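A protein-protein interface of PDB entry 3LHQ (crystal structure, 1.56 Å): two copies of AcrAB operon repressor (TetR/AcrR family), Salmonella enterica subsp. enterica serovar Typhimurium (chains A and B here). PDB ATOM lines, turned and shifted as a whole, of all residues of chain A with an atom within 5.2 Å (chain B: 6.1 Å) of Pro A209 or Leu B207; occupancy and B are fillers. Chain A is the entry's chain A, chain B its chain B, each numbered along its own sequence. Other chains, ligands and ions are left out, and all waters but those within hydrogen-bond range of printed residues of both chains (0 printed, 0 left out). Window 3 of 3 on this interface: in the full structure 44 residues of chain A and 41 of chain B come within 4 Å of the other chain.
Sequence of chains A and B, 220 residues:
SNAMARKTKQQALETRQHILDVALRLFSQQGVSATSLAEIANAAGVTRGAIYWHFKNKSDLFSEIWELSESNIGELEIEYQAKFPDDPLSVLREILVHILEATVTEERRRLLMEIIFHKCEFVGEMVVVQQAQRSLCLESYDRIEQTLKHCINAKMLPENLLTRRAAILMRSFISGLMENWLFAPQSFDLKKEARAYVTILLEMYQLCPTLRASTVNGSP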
ATOM      1  N   LEU A 207      16.362 -17.051 -29.687  1.00  0.00           N
ATOM      2  CA  LEU A 207      15.571 -15.850 -29.439  1.00  0.00           C
ATOM      3  C   LEU A 207      16.068 -14.563 -30.071  1.00  0.00           C
ATOM      4  O   LEU A 207      15.257 -13.698 -30.391  1.00  0.00           O
ATOM      5  CB  LEU A 207      15.397 -15.598 -27.921  1.00  0.00           C
ATOM      6  CG  LEU A 207      14.800 -16.717 -27.096  1.00  0.00           C
ATOM      7  CD1 LEU A 207      15.050 -16.410 -25.602  1.00  0.00           C
ATOM      8  CD2 LEU A 207      13.317 -16.867 -27.467  1.00  0.00           C
ATOM      9  N   CYS A 208      17.374 -14.365 -30.221  1.00  0.00           N
ATOM     10  CA  CYS A 208      17.831 -13.006 -30.571  1.00  0.00           C
ATOM     11  C   CYS A 208      17.594 -12.738 -32.058  1.00  0.00           C
ATOM     12  O   CYS A 208      18.106 -13.454 -32.920  1.00  0.00           O
ATOM     13  CB  CYS A 208      19.322 -12.836 -30.253  1.00  0.00           C
ATOM     14  SG  CYS A 208      19.721 -12.971 -28.497  1.00  0.00           S
ATOM     15  N   PRO A 209      16.817 -11.726 -32.382  1.00  0.00           N
ATOM     16  CA  PRO A 209      16.490 -11.475 -33.807  1.00  0.00           C
ATOM     17  C   PRO A 209      17.684 -11.154 -34.731  1.00  0.00           C
ATOM     18  O   PRO A 209      17.613 -11.516 -35.919  1.00  0.00           O
ATOM     19  CB  PRO A 209      15.490 -10.310 -33.746  1.00  0.00           C
ATOM     20  CG  PRO A 209      15.655  -9.699 -32.454  1.00  0.00           C
ATOM     21  CD  PRO A 209      16.140 -10.778 -31.490  1.00  0.00           C
ATOM     22  N   THR A 210      18.784 -10.572 -34.205  1.00  0.00           N
ATOM     23  CA  THR A 210      19.920 -10.301 -35.037  1.00  0.00           C
ATOM     24  C   THR A 210      20.725 -11.545 -35.366  1.00  0.00           C
ATOM     25  O   THR A 210      21.685 -11.468 -36.096  1.00  0.00           O
ATOM     26  CB  THR A 210      20.687  -9.164 -34.408  1.00  0.00           C
ATOM     27  OG1 THR A 210      19.766  -8.056 -34.293  1.00  0.00           O
ATOM     28  CG2 THR A 210      21.940  -8.753 -35.196  1.00  0.00           C
ATOM     29  N   LEU A 211      20.363 -12.698 -34.789  1.00  0.00           N
ATOM     30  CA  LEU A 211      20.883 -13.976 -35.219  1.00  0.00           C
ATOM     31  C   LEU A 211      20.087 -14.630 -36.342  1.00  0.00           C
ATOM     32  O   LEU A 211      20.430 -15.743 -36.712  1.00  0.00           O
ATOM     33  CB  LEU A 211      21.043 -14.958 -34.039  1.00  0.00           C
ATOM     34  CG  LEU A 211      22.407 -14.708 -33.338  1.00  0.00           C
ATOM     35  CD1 LEU A 211      22.525 -15.453 -32.012  1.00  0.00           C
ATOM     36  CD2 LEU A 211      23.590 -15.066 -34.307  1.00  0.00           C
ATOM     37  N   ARG A 212      19.066 -13.953 -36.872  1.00  0.00           N
ATOM     38  CA  ARG A 212      18.289 -14.534 -37.961  1.00  0.00           C
ATOM     39  C   ARG A 212      18.330 -13.681 -39.212  1.00  0.00           C
ATOM     40  O   ARG A 212      18.493 -12.437 -39.164  1.00  0.00           O
ATOM     41  CB  ARG A 212      16.869 -14.768 -37.554  1.00  0.00           C
ATOM     42  CG  ARG A 212      16.791 -15.708 -36.355  1.00  0.00           C
ATOM     43  CD  ARG A 212      15.388 -16.034 -35.922  1.00  0.00           C
ATOM     44  NE  ARG A 212      14.745 -14.901 -35.258  1.00  0.00           N
ATOM     45  CZ  ARG A 212      13.743 -14.996 -34.387  1.00  0.00           C
ATOM     46  NH1 ARG A 212      13.241 -16.199 -34.047  1.00  0.00           N
ATOM     47  NH2 ARG A 212      13.255 -13.886 -33.819  1.00  0.00           N
ATOM     48  N   PRO B 158      15.592  -5.591 -18.577  1.00  0.00           N
ATOM     49  CA  PRO B 158      14.573  -6.171 -17.697  1.00  0.00           C
ATOM     50  C   PRO B 158      14.846  -5.934 -16.224  1.00  0.00           C
ATOM     51  O   PRO B 158      15.976  -5.988 -15.752  1.00  0.00           O
ATOM     52  CB  PRO B 158      14.600  -7.700 -18.033  1.00  0.00           C
ATOM     53  CG  PRO B 158      15.159  -7.727 -19.395  1.00  0.00           C
ATOM     54  CD  PRO B 158      16.208  -6.615 -19.437  1.00  0.00           C
ATOM     55  N   LEU B 202      23.169  -7.311 -26.485  1.00  0.00           N
ATOM     56  CA  LEU B 202      22.105  -6.547 -25.808  1.00  0.00           C
ATOM     57  C   LEU B 202      20.725  -7.221 -25.930  1.00  0.00           C
ATOM     58  O   LEU B 202      19.931  -7.190 -24.988  1.00  0.00           O
ATOM     59  CB  LEU B 202      22.105  -5.091 -26.332  1.00  0.00           C
ATOM     60  CG  LEU B 202      23.446  -4.359 -26.145  1.00  0.00           C
ATOM     61  CD1 LEU B 202      23.384  -2.930 -26.637  1.00  0.00           C
ATOM     62  CD2 LEU B 202      23.952  -4.303 -24.691  1.00  0.00           C
ATOM     63  N   GLU B 203      20.451  -7.852 -27.080  1.00  0.00           N
ATOM     64  CA  GLU B 203      19.285  -8.671 -27.256  1.00  0.00           C
ATOM     65  C   GLU B 203      19.250  -9.829 -26.233  1.00  0.00           C
ATOM     66  O   GLU B 203      18.189 -10.128 -25.711  1.00  0.00           O
ATOM     67  CB  GLU B 203      19.176  -9.181 -28.665  1.00  0.00           C
ATOM     68  CG  GLU B 203      18.792  -8.140 -29.704  1.00  0.00           C
ATOM     69  CD  GLU B 203      18.932  -8.610 -31.133  1.00  0.00           C
ATOM     70  OE1 GLU B 203      19.333  -9.802 -31.390  1.00  0.00           O
ATOM     71  OE2 GLU B 203      18.630  -7.766 -32.036  1.00  0.00           O
ATOM     72  N   MET B 204      20.406 -10.434 -25.942  1.00  0.00           N
ATOM     73  CA  MET B 204      20.489 -11.474 -24.930  1.00  0.00           C
ATOM     74  C   MET B 204      20.045 -10.964 -23.578  1.00  0.00           C
ATOM     75  O   MET B 204      19.264 -11.622 -22.902  1.00  0.00           O
ATOM     76  CB  MET B 204      21.904 -12.016 -24.804  1.00  0.00           C
ATOM     77  CG  MET B 204      22.318 -12.817 -25.986  1.00  0.00           C
ATOM     78  SD  MET B 204      24.041 -13.059 -26.023  1.00  0.00           S
ATOM     79  CE  MET B 204      24.085 -14.852 -26.312  1.00  0.00           C
ATOM     80  N   TYR B 205      20.489  -9.759 -23.189  1.00  0.00           N
ATOM     81  CA  TYR B 205      20.034  -9.148 -21.948  1.00  0.00           C
ATOM     82  C   TYR B 205      18.549  -8.958 -21.917  1.00  0.00           C
ATOM     83  O   TYR B 205      17.946  -9.056 -20.846  1.00  0.00           O
ATOM     84  CB  TYR B 205      20.776  -7.806 -21.755  1.00  0.00           C
ATOM     85  CG  TYR B 205      22.285  -7.899 -21.469  1.00  0.00           C
ATOM     86  CD1 TYR B 205      22.914  -9.088 -21.050  1.00  0.00           C
ATOM     87  CD2 TYR B 205      23.120  -6.815 -21.729  1.00  0.00           C
ATOM     88  CE1 TYR B 205      24.291  -9.163 -20.822  1.00  0.00           C
ATOM     89  CE2 TYR B 205      24.485  -6.870 -21.490  1.00  0.00           C
ATOM     90  CZ  TYR B 205      25.058  -8.035 -21.027  1.00  0.00           C
ATOM     91  OH  TYR B 205      26.380  -8.124 -20.824  1.00  0.00           O
ATOM     92  N   GLN B 206      17.981  -8.559 -23.060  1.00  0.00           N
ATOM     93  CA  GLN B 206      16.561  -8.269 -23.133  1.00  0.00           C
ATOM     94  C   GLN B 206      15.720  -9.552 -23.144  1.00  0.00           C
ATOM     95  O   GLN B 206      14.620  -9.586 -22.602  1.00  0.00           O
ATOM     96  CB  GLN B 206      16.238  -7.494 -24.398  1.00  0.00           C
ATOM     97  CG  GLN B 206      16.897  -6.204 -24.506  1.00  0.00           C
ATOM     98  CD  GLN B 206      16.232  -5.118 -23.722  1.00  0.00           C
ATOM     99  OE1 GLN B 206      15.607  -5.379 -22.683  1.00  0.00           O
ATOM    100  NE2 GLN B 206      16.346  -3.866 -24.220  1.00  0.00           N
ATOM    101  N   LEU B 207      16.251 -10.621 -23.730  1.00  0.00           N
ATOM    102  CA  LEU B 207      15.411 -11.757 -24.060  1.00  0.00           C
ATOM    103  C   LEU B 207      15.708 -13.054 -23.340  1.00  0.00           C
ATOM    104  O   LEU B 207      14.789 -13.872 -23.197  1.00  0.00           O
ATOM    105  CB  LEU B 207      15.391 -12.008 -25.572  1.00  0.00           C
ATOM    106  CG  LEU B 207      15.020 -10.772 -26.432  1.00  0.00           C
ATOM    107  CD1 LEU B 207      15.267 -11.099 -27.928  1.00  0.00           C
ATOM    108  CD2 LEU B 207      13.560 -10.381 -26.161  1.00  0.00           C
ATOM    109  N   CYS B 208      16.976 -13.350 -23.043  1.00  0.00           N
ATOM    110  CA  CYS B 208      17.262 -14.715 -22.573  1.00  0.00           C
ATOM    111  C   CYS B 208      16.793 -14.958 -21.145  1.00  0.00           C
ATOM    112  O   CYS B 208      17.197 -14.290 -20.239  1.00  0.00           O
ATOM    113  CB  CYS B 208      18.744 -14.958 -22.718  1.00  0.00           C
ATOM    114  SG  CYS B 208      19.397 -14.948 -24.396  1.00  0.00           S
ATOM    115  N   PRO B 209      15.881 -15.914 -20.939  1.00  0.00           N
ATOM    116  CA  PRO B 209      15.335 -16.140 -19.611  1.00  0.00           C
ATOM    117  C   PRO B 209      16.332 -16.563 -18.550  1.00  0.00           C
ATOM    118  O   PRO B 209      16.128 -16.238 -17.372  1.00  0.00           O
ATOM    119  CB  PRO B 209      14.275 -17.226 -19.863  1.00  0.00           C
ATOM    120  CG  PRO B 209      14.474 -17.699 -21.119  1.00  0.00           C
ATOM    121  CD  PRO B 209      15.191 -16.744 -21.946  1.00  0.00           C
ATOM    122  N   THR B 210      17.453 -17.183 -18.930  1.00  0.00           N
ATOM    123  CA  THR B 210      18.407 -17.581 -17.915  1.00  0.00           C
ATOM    124  C   THR B 210      19.298 -16.447 -17.420  1.00  0.00           C
ATOM    125  O   THR B 210      20.146 -16.635 -16.537  1.00  0.00           O
ATOM    126  CB  THR B 210      19.141 -18.849 -18.440  1.00  0.00           C
ATOM    127  OG1 THR B 210      18.149 -19.885 -18.587  1.00  0.00           O
ATOM    128  CG2 THR B 210      20.211 -19.375 -17.515  1.00  0.00           C
ATOM    129  N   ARG B 212      17.757 -13.883 -16.208  1.00  0.00           N
ATOM    130  CA  ARG B 212      16.859 -13.279 -15.242  1.00  0.00           C
ATOM    131  C   ARG B 212      16.654 -14.078 -14.004  1.00  0.00           C
ATOM    132  O   ARG B 212      16.673 -15.344 -14.038  1.00  0.00           O
ATOM    133  CB  ARG B 212      15.535 -13.115 -15.908  1.00  0.00           C
ATOM    134  CG  ARG B 212      15.605 -12.154 -17.089  1.00  0.00           C
ATOM    135  CD  ARG B 212      14.253 -12.176 -17.664  1.00  0.00           C
ATOM    136  NE  ARG B 212      14.064 -11.296 -18.791  1.00  0.00           N
ATOM    137  CZ  ARG B 212      13.164 -11.544 -19.740  1.00  0.00           C
ATOM    138  NH1 ARG B 212      12.457 -12.687 -19.736  1.00  0.00           N
ATOM    139  NH2 ARG B 212      12.976 -10.670 -20.713  1.00  0.00           N
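CD1 of Leu A207 touches O of Leu B207, at 3.5 Å.
Leu A207 touches Pro B209.
Glu B203 touches Cys A208.
Pro A209 touches Leu B207.
SG of Cys A208 lies close to N of Met B204.
The side-chain hydroxyl (OG1) of Thr A210 sits at hydrogen-bond distance from the side-chain carboxylate (OE2) of Glu B203 (2.5 Å).
The backbone nitrogen (N) of Pro A209 sits close to the side-chain carboxylate (OE1) of Glu B203 (3.3 Å).
Pro A209 touches just these residues of chain B: Glu B203 (3.3 Å) and Leu B207 (3.7 Å).
Of chain A, only Leu A207 and Pro A209 come within 4 Å of Leu B207.
Printed residues of chain A within 4 Å of Glu B203: Cys A208, Pro A209 and Thr A210.
Of the printed residues of chain A, Met B204 touches Cys A208.
Of the printed residues of chain A, Pro B209 touches Leu A207 (3.7 Å).
The nearest residue of chain A that does not touch Leu B207 is Cys A208 (4.1 Å).
Printed residues of chain B that touch a printed residue of chain A: Glu B203, Met B204, Leu B207 and Pro B209.
Hydrophobic or aromatic side chains of chain B within 4 Å of the printed part of chain A: Met B204, Leu B207 and Pro B209.
Along chain B the printed residues that touch a printed residue of chain A span positions 203 to 209.
Hydrophobic or aromatic side chains of chain A within 4 Å of the printed part of chain B: Leu A207 and Pro A209.
Among the printed residues, no Asp or Glu carboxylate lies within 4 Å of a Lys or Arg side-chain nitrogen of the other chain.
The side-chain sulfur of Cys B208 lies close to the backbone carbonyl oxygen of Met B204.
Leu B207 touches its own counterpart, Leu A207.
Leu A207 touches Pro B209, and with the chains exchanged Pro A209 touches Leu B207.
Positions printed for both chains: 207, 208, 209, 210 and 212.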
